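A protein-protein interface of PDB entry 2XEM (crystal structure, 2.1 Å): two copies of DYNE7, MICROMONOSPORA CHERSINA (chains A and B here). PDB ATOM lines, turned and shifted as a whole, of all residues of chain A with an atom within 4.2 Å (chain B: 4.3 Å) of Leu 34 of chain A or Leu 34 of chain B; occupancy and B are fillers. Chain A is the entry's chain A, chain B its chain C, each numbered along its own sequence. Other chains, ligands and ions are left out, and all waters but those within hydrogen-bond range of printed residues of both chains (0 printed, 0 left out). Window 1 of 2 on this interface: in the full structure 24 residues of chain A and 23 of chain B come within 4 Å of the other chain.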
ATOM      1  N   PHE A  30      26.734 -18.906  26.029  1.00  0.00           N
ATOM      2  CA  PHE A  30      26.082 -20.111  25.456  1.00  0.00           C
ATOM      3  C   PHE A  30      26.069 -20.155  23.923  1.00  0.00           C
ATOM      4  O   PHE A  30      26.238 -21.217  23.350  1.00  0.00           O
ATOM      5  CB  PHE A  30      24.651 -20.296  26.028  1.00  0.00           C
ATOM      6  CG  PHE A  30      23.621 -19.391  25.374  1.00  0.00           C
ATOM      7  CD1 PHE A  30      22.838 -19.849  24.318  1.00  0.00           C
ATOM      8  CD2 PHE A  30      23.458 -18.072  25.791  1.00  0.00           C
ATOM      9  CE1 PHE A  30      21.916 -19.004  23.691  1.00  0.00           C
ATOM     10  CE2 PHE A  30      22.543 -17.226  25.157  1.00  0.00           C
ATOM     11  CZ  PHE A  30      21.776 -17.704  24.112  1.00  0.00           C
ATOM     12  N   ALA A  31      25.832 -18.999  23.267  1.00  0.00           N
ATOM     13  CA  ALA A  31      25.682 -18.913  21.818  1.00  0.00           C
ATOM     14  C   ALA A  31      26.931 -19.323  21.037  1.00  0.00           C
ATOM     15  O   ALA A  31      26.789 -19.760  19.892  1.00  0.00           O
ATOM     16  CB  ALA A  31      25.219 -17.525  21.401  1.00  0.00           C
ATOM     17  N   HIS A  32      28.140 -19.196  21.629  1.00  0.00           N
ATOM     18  CA  HIS A  32      29.396 -19.662  20.997  1.00  0.00           C
ATOM     19  C   HIS A  32      29.428 -21.135  20.642  1.00  0.00           C
ATOM     20  O   HIS A  32      30.005 -21.491  19.624  1.00  0.00           O
ATOM     21  CB  HIS A  32      30.655 -19.217  21.757  1.00  0.00           C
ATOM     22  CG  HIS A  32      30.725 -17.727  21.870  1.00  0.00           C
ATOM     23  ND1 HIS A  32      30.794 -16.921  20.745  1.00  0.00           N
ATOM     24  CD2 HIS A  32      30.643 -16.945  22.969  1.00  0.00           C
ATOM     25  CE1 HIS A  32      30.785 -15.678  21.193  1.00  0.00           C
ATOM     26  NE2 HIS A  32      30.714 -15.638  22.528  1.00  0.00           N
ATOM     27  N   TYR A  33      28.780 -21.979  21.450  1.00  0.00           N
ATOM     28  CA  TYR A  33      28.656 -23.410  21.194  1.00  0.00           C
ATOM     29  C   TYR A  33      27.965 -23.693  19.854  1.00  0.00           C
ATOM     30  O   TYR A  33      28.279 -24.688  19.198  1.00  0.00           O
ATOM     31  CB  TYR A  33      27.878 -24.086  22.343  1.00  0.00           C
ATOM     32  CG  TYR A  33      28.644 -24.174  23.643  1.00  0.00           C
ATOM     33  CD1 TYR A  33      29.245 -25.368  24.041  1.00  0.00           C
ATOM     34  CD2 TYR A  33      28.739 -23.073  24.498  1.00  0.00           C
ATOM     35  CE1 TYR A  33      29.908 -25.477  25.273  1.00  0.00           C
ATOM     36  CE2 TYR A  33      29.406 -23.164  25.725  1.00  0.00           C
ATOM     37  CZ  TYR A  33      29.984 -24.373  26.108  1.00  0.00           C
ATOM     38  OH  TYR A  33      30.631 -24.501  27.310  1.00  0.00           O
ATOM     39  N   LEU A  34      27.021 -22.834  19.452  1.00  0.00           N
ATOM     40  CA  LEU A  34      26.360 -22.946  18.144  1.00  0.00           C
ATOM     41  C   LEU A  34      27.266 -22.524  17.031  1.00  0.00           C
ATOM     42  O   LEU A  34      27.248 -23.181  16.014  1.00  0.00           O
ATOM     43  CB  LEU A  34      24.999 -22.200  18.078  1.00  0.00           C
ATOM     44  CG  LEU A  34      23.812 -22.836  18.854  1.00  0.00           C
ATOM     45  CD1 LEU A  34      23.687 -24.353  18.584  1.00  0.00           C
ATOM     46  CD2 LEU A  34      23.904 -22.569  20.360  1.00  0.00           C
ATOM     47  N   HIS A  35      28.074 -21.446  17.204  1.00  0.00           N
ATOM     48  CA  HIS A  35      29.086 -21.073  16.210  1.00  0.00           C
ATOM     49  C   HIS A  35      30.021 -22.233  15.951  1.00  0.00           C
ATOM     50  O   HIS A  35      30.344 -22.505  14.795  1.00  0.00           O
ATOM     51  CB  HIS A  35      29.908 -19.844  16.641  1.00  0.00           C
ATOM     52  CG  HIS A  35      29.151 -18.564  16.617  1.00  0.00           C
ATOM     53  ND1 HIS A  35      29.236 -17.690  15.545  1.00  0.00           N
ATOM     54  CD2 HIS A  35      28.346 -18.024  17.554  1.00  0.00           C
ATOM     55  CE1 HIS A  35      28.482 -16.660  15.857  1.00  0.00           C
ATOM     56  NE2 HIS A  35      27.905 -16.822  17.049  1.00  0.00           N
ATOM     57  N   TRP A  36      30.430 -22.937  17.016  1.00  0.00           N
ATOM     58  CA  TRP A  36      31.389 -24.043  16.921  1.00  0.00           C
ATOM     59  C   TRP A  36      30.878 -25.211  16.080  1.00  0.00           C
ATOM     60  O   TRP A  36      31.696 -25.924  15.498  1.00  0.00           O
ATOM     61  CB  TRP A  36      31.771 -24.536  18.315  1.00  0.00           C
ATOM     62  CG  TRP A  36      32.482 -23.539  19.190  1.00  0.00           C
ATOM     63  CD1 TRP A  36      33.030 -22.349  18.820  1.00  0.00           C
ATOM     64  CD2 TRP A  36      32.673 -23.649  20.606  1.00  0.00           C
ATOM     65  NE1 TRP A  36      33.543 -21.703  19.919  1.00  0.00           N
ATOM     66  CE2 TRP A  36      33.341 -22.479  21.031  1.00  0.00           C
ATOM     67  CE3 TRP A  36      32.358 -24.642  21.562  1.00  0.00           C
ATOM     68  CZ2 TRP A  36      33.687 -22.256  22.374  1.00  0.00           C
ATOM     69  CZ3 TRP A  36      32.696 -24.424  22.895  1.00  0.00           C
ATOM     70  CH2 TRP A  36      33.360 -23.249  23.292  1.00  0.00           C
ATOM     71  N   GLN A  37      29.542 -25.407  16.015  1.00  0.00           N
ATOM     72  CA  GLN A  37      28.896 -26.395  15.119  1.00  0.00           C
ATOM     73  C   GLN A  37      29.206 -26.057  13.662  1.00  0.00           C
ATOM     74  O   GLN A  37      29.562 -26.942  12.890  1.00  0.00           O
ATOM     75  CB  GLN A  37      27.384 -26.416  15.342  1.00  0.00           C
ATOM     76  CG  GLN A  37      26.980 -27.038  16.664  1.00  0.00           C
ATOM     77  CD  GLN A  37      25.488 -27.160  16.849  1.00  0.00           C
ATOM     78  OE1 GLN A  37      24.690 -26.856  15.960  1.00  0.00           O
ATOM     79  NE2 GLN A  37      25.082 -27.645  18.018  1.00  0.00           N
ATOM     80  N   GLY A  38      29.081 -24.769  13.332  1.00  0.00           N
ATOM     81  CA  GLY A  38      29.419 -24.226  12.024  1.00  0.00           C
ATOM     82  C   GLY A  38      30.892 -24.385  11.722  1.00  0.00           C
ATOM     83  O   GLY A  38      31.247 -24.861  10.651  1.00  0.00           O
ATOM     84  N   CYS A  67      18.659 -26.096  14.990  1.00  0.00           N
ATOM     85  CA  CYS A  67      19.818 -26.418  15.813  1.00  0.00           C
ATOM     86  C   CYS A  67      19.394 -26.468  17.279  1.00  0.00           C
ATOM     87  O   CYS A  67      18.360 -25.913  17.660  1.00  0.00           O
ATOM     88  CB  CYS A  67      20.970 -25.441  15.585  1.00  0.00           C
ATOM     89  SG  CYS A  67      20.626 -23.765  16.152  1.00  0.00           S
ATOM     90  N   HIS A  68      20.223 -27.089  18.094  1.00  0.00           N
ATOM     91  CA  HIS A  68      19.915 -27.410  19.489  1.00  0.00           C
ATOM     92  C   HIS A  68      21.225 -27.563  20.263  1.00  0.00           C
ATOM     93  O   HIS A  68      22.213 -28.002  19.697  1.00  0.00           O
ATOM     94  CB  HIS A  68      19.094 -28.717  19.586  1.00  0.00           C
ATOM     95  CG  HIS A  68      18.426 -28.877  20.915  1.00  0.00           C
ATOM     96  ND1 HIS A  68      19.069 -29.509  21.976  1.00  0.00           N
ATOM     97  CD2 HIS A  68      17.221 -28.427  21.340  1.00  0.00           C
ATOM     98  CE1 HIS A  68      18.220 -29.438  22.987  1.00  0.00           C
ATOM     99  NE2 HIS A  68      17.102 -28.785  22.647  1.00  0.00           N
ATOM    100  N   PHE B  30      23.177 -18.394  11.037  1.00  0.00           N
ATOM    101  CA  PHE B  30      22.174 -19.010  11.930  1.00  0.00           C
ATOM    102  C   PHE B  30      22.440 -18.753  13.437  1.00  0.00           C
ATOM    103  O   PHE B  30      21.489 -18.571  14.190  1.00  0.00           O
ATOM    104  CB  PHE B  30      22.029 -20.544  11.648  1.00  0.00           C
ATOM    105  CG  PHE B  30      23.131 -21.380  12.281  1.00  0.00           C
ATOM    106  CD1 PHE B  30      22.950 -21.974  13.534  1.00  0.00           C
ATOM    107  CD2 PHE B  30      24.365 -21.524  11.653  1.00  0.00           C
ATOM    108  CE1 PHE B  30      23.983 -22.705  14.132  1.00  0.00           C
ATOM    109  CE2 PHE B  30      25.386 -22.274  12.246  1.00  0.00           C
ATOM    110  CZ  PHE B  30      25.195 -22.846  13.484  1.00  0.00           C
ATOM    111  N   ALA B  31      23.717 -18.759  13.860  1.00  0.00           N
ATOM    112  CA  ALA B  31      24.091 -18.666  15.277  1.00  0.00           C
ATOM    113  C   ALA B  31      23.702 -17.323  15.928  1.00  0.00           C
ATOM    114  O   ALA B  31      23.505 -17.284  17.129  1.00  0.00           O
ATOM    115  CB  ALA B  31      25.568 -18.951  15.455  1.00  0.00           C
ATOM    116  N   HIS B  32      23.600 -16.240  15.140  1.00  0.00           N
ATOM    117  CA  HIS B  32      23.133 -14.930  15.615  1.00  0.00           C
ATOM    118  C   HIS B  32      21.749 -14.926  16.212  1.00  0.00           C
ATOM    119  O   HIS B  32      21.517 -14.187  17.166  1.00  0.00           O
ATOM    120  CB  HIS B  32      23.318 -13.823  14.567  1.00  0.00           C
ATOM    121  CG  HIS B  32      24.748 -13.695  14.138  1.00  0.00           C
ATOM    122  ND1 HIS B  32      25.746 -13.378  15.049  1.00  0.00           N
ATOM    123  CD2 HIS B  32      25.318 -13.921  12.926  1.00  0.00           C
ATOM    124  CE1 HIS B  32      26.882 -13.388  14.360  1.00  0.00           C
ATOM    125  NE2 HIS B  32      26.669 -13.686  13.070  1.00  0.00           N
ATOM    126  N   TYR B  33      20.842 -15.776  15.701  1.00  0.00           N
ATOM    127  CA  TYR B  33      19.496 -15.950  16.259  1.00  0.00           C
ATOM    128  C   TYR B  33      19.542 -16.366  17.734  1.00  0.00           C
ATOM    129  O   TYR B  33      18.663 -15.992  18.507  1.00  0.00           O
ATOM    130  CB  TYR B  33      18.687 -16.971  15.431  1.00  0.00           C
ATOM    131  CG  TYR B  33      18.290 -16.465  14.051  1.00  0.00           C
ATOM    132  CD1 TYR B  33      16.988 -16.034  13.789  1.00  0.00           C
ATOM    133  CD2 TYR B  33      19.202 -16.468  12.994  1.00  0.00           C
ATOM    134  CE1 TYR B  33      16.598 -15.633  12.506  1.00  0.00           C
ATOM    135  CE2 TYR B  33      18.824 -16.071  11.712  1.00  0.00           C
ATOM    136  CZ  TYR B  33      17.520 -15.656  11.473  1.00  0.00           C
ATOM    137  OH  TYR B  33      17.141 -15.251  10.222  1.00  0.00           O
ATOM    138  N   LEU B  34      20.554 -17.151  18.115  1.00  0.00           N
ATOM    139  CA  LEU B  34      20.753 -17.546  19.520  1.00  0.00           C
ATOM    140  C   LEU B  34      21.259 -16.406  20.366  1.00  0.00           C
ATOM    141  O   LEU B  34      20.785 -16.260  21.470  1.00  0.00           O
ATOM    142  CB  LEU B  34      21.637 -18.811  19.670  1.00  0.00           C
ATOM    143  CG  LEU B  34      20.977 -20.167  19.253  1.00  0.00           C
ATOM    144  CD1 LEU B  34      19.558 -20.330  19.844  1.00  0.00           C
ATOM    145  CD2 LEU B  34      20.949 -20.365  17.724  1.00  0.00           C
ATOM    146  N   HIS B  35      22.188 -15.563  19.847  1.00  0.00           N
ATOM    147  CA  HIS B  35      22.625 -14.361  20.569  1.00  0.00           C
ATOM    148  C   HIS B  35      21.434 -13.471  20.863  1.00  0.00           C
ATOM    149  O   HIS B  35      21.345 -12.927  21.958  1.00  0.00           O
ATOM    150  CB  HIS B  35      23.659 -13.530  19.753  1.00  0.00           C
ATOM    151  CG  HIS B  35      24.994 -14.167  19.648  1.00  0.00           C
ATOM    152  ND1 HIS B  35      26.028 -13.801  20.479  1.00  0.00           N
ATOM    153  CD2 HIS B  35      25.438 -15.106  18.790  1.00  0.00           C
ATOM    154  CE1 HIS B  35      27.065 -14.515  20.100  1.00  0.00           C
ATOM    155  NE2 HIS B  35      26.755 -15.321  19.093  1.00  0.00           N
ATOM    156  N   TRP B  36      20.505 -13.349  19.913  1.00  0.00           N
ATOM    157  CA  TRP B  36      19.328 -12.468  20.046  1.00  0.00           C
ATOM    158  C   TRP B  36      18.396 -12.877  21.189  1.00  0.00           C
ATOM    159  O   TRP B  36      17.706 -12.021  21.737  1.00  0.00           O
ATOM    160  CB  TRP B  36      18.542 -12.414  18.737  1.00  0.00           C
ATOM    161  CG  TRP B  36      19.302 -11.844  17.565  1.00  0.00           C
ATOM    162  CD1 TRP B  36      20.503 -11.189  17.589  1.00  0.00           C
ATOM    163  CD2 TRP B  36      18.918 -11.932  16.187  1.00  0.00           C
ATOM    164  NE1 TRP B  36      20.891 -10.870  16.312  1.00  0.00           N
ATOM    165  CE2 TRP B  36      19.947 -11.325  15.427  1.00  0.00           C
ATOM    166  CE3 TRP B  36      17.791 -12.466  15.513  1.00  0.00           C
ATOM    167  CZ2 TRP B  36      19.879 -11.209  14.030  1.00  0.00           C
ATOM    168  CZ3 TRP B  36      17.744 -12.379  14.126  1.00  0.00           C
ATOM    169  CH2 TRP B  36      18.774 -11.748  13.402  1.00  0.00           C
ATOM    170  N   GLN B  37      18.371 -14.174  21.537  1.00  0.00           N
ATOM    171  CA  GLN B  37      17.654 -14.692  22.707  1.00  0.00           C
ATOM    172  C   GLN B  37      18.235 -14.094  23.986  1.00  0.00           C
ATOM    173  O   GLN B  37      17.486 -13.671  24.870  1.00  0.00           O
ATOM    174  CB  GLN B  37      17.754 -16.223  22.744  1.00  0.00           C
ATOM    175  CG  GLN B  37      16.943 -16.900  21.648  1.00  0.00           C
ATOM    176  CD  GLN B  37      16.957 -18.401  21.750  1.00  0.00           C
ATOM    177  OE1 GLN B  37      17.528 -18.991  22.678  1.00  0.00           O
ATOM    178  NE2 GLN B  37      16.332 -19.059  20.785  1.00  0.00           N
ATOM    179  N   GLY B  38      19.561 -14.060  24.056  1.00  0.00           N
ATOM    180  CA  GLY B  38      20.296 -13.434  25.133  1.00  0.00           C
ATOM    181  C   GLY B  38      20.035 -11.953  25.217  1.00  0.00           C
ATOM    182  O   GLY B  38      19.736 -11.446  26.303  1.00  0.00           O
ATOM    183  N   CYS B  67      18.990 -24.657  24.541  1.00  0.00           N
ATOM    184  CA  CYS B  67      18.439 -23.705  23.585  1.00  0.00           C
ATOM    185  C   CYS B  67      18.158 -24.430  22.273  1.00  0.00           C
ATOM    186  O   CYS B  67      18.692 -25.513  22.034  1.00  0.00           O
ATOM    187  CB  CYS B  67      19.348 -22.496  23.384  1.00  0.00           C
ATOM    188  SG  CYS B  67      20.917 -22.882  22.568  1.00  0.00           S
ATOM    189  N   HIS B  68      17.325 -23.810  21.427  1.00  0.00           N
ATOM    190  CA  HIS B  68      16.791 -24.395  20.211  1.00  0.00           C
ATOM    191  C   HIS B  68      16.385 -23.259  19.274  1.00  0.00           C
ATOM    192  O   HIS B  68      15.968 -22.194  19.721  1.00  0.00           O
ATOM    193  CB  HIS B  68      15.569 -25.300  20.530  1.00  0.00           C
ATOM    194  CG  HIS B  68      15.229 -26.213  19.402  1.00  0.00           C
ATOM    195  ND1 HIS B  68      14.350 -25.827  18.400  1.00  0.00           N
ATOM    196  CD2 HIS B  68      15.700 -27.448  19.117  1.00  0.00           C
ATOM    197  CE1 HIS B  68      14.310 -26.845  17.562  1.00  0.00           C
ATOM    198  NE2 HIS B  68      15.117 -27.836  17.947  1.00  0.00           N
ATOM    199  N   ALA B  69      16.545 -23.480  17.968  1.00  0.00           N
ATOM    200  CA  ALA B  69      16.014 -22.593  16.935  1.00  0.00           C
ATOM    201  C   ALA B  69      15.538 -23.414  15.743  1.00  0.00           C
ATOM    202  O   ALA B  69      16.159 -24.421  15.412  1.00  0.00           O
ATOM    203  CB  ALA B  69      17.065 -21.574  16.494  1.00  0.00           C
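Ala 31 of chain A touches His 35 of chain B, and with the chains exchanged His 35 of chain A touches Ala 31 of chain B. Leu 34 of chain A touches Cys 67 of chain B, and with the chains exchanged Cys 67 of chain A touches Leu 34 of chain B. Cys 67 of chain A touches His 68 of chain B, and with the chains exchanged His 68 of chain A touches Cys 67 of chain B. His 68 of chain A touches its own counterpart, His 68 of chain B. Of the 15 pairs that touch across the chains among the printed residues, 13 have their exchanged pair printed and touching as well.
Among the printed residues, merely in contact across the chains: Phe 30 of chain A with Leu 34 of chain B, Phe 30 of chain A with Cys 67 of chain B, Ala 31 of chain A with His 35 of chain B, Leu 34 of chain A with Phe 30 of chain B, Leu 34 of chain A with Leu 34 of chain B, Leu 34 of chain A with Cys 67 of chain B, His 35 of chain A with Ala 31 of chain B, His 35 of chain A with His 32 of chain B, Cys 67 of chain A with Phe 30 of chain B, Cys 67 of chain A with Leu 34 of chain B, Cys 67 of chain A with His 68 of chain B, His 68 of chain A with Cys 67 of chain B and His 68 of chain A with His 68 of chain B.
NE2 of His 35 of chain B lies within hydrogen-bond range of NE2 of His 35 of chain A (2.8 Å). N of Cys 67 of chain A is in hydrogen-bond range of O of Ala 69 of chain B (3.0 Å).
Of chain B, only Phe 30, Leu 34 and Cys 67 come within 4 Å of Leu 34 of chain A. Of the printed residues of chain B, Cys 67 of chain A touches Phe 30, Leu 34, His 68 and Ala 69. Of the printed residues of chain B, His 68 of chain A touches Cys 67 and His 68. Leu 34 of chain B touches just these residues of chain A: Phe 30 (3.2 Å), Leu 34 (3.9 Å) and Cys 67 (3.8 Å). The nearest printed residue of chain A that does not touch Leu 34 of chain B is Ala 31 of chain A (4.2 Å). The nearest printed residue of chain B that does not touch Phe 30 of chain A is Gly 38 of chain B (4.3 Å).
The side-chain amide nitrogen (NE2) of Gln 37 of chain A lies within hydrogen-bond range of the backbone carbonyl oxygen (O) of His 68 of chain A, at 3.3 Å. The indole nitrogen of Trp 36 of chain B sits close to the backbone carbonyl oxygen of His 32 of chain B, 3.5 Å away. The side-chain amide nitrogen (NE2) of Gln 37 of chain B is in hydrogen-bond range of the backbone carbonyl oxygen (O) of His 68 of chain B (3.3 Å).
Of the 12 printed residues of chain B, 8 touch a printed residue of chain A. Hydrophobic or aromatic side chains of chain B within 4 Å of the printed part of chain A: Phe 30, Ala 31, His 32, Leu 34, His 35 and His 68. Of the 11 printed residues of chain A, 6 touch a printed residue of chain B. Hydrophobic or aromatic side chains of chain A that line the printed part of chain B: Phe 30, Ala 31, Leu 34, His 35 and His 68. Among the printed residues, 15 pairs touch across the chains. Among the printed residues, no Asp or Glu carboxylate lies within 4 Å of a Lys or Arg side-chain nitrogen of the other chain.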
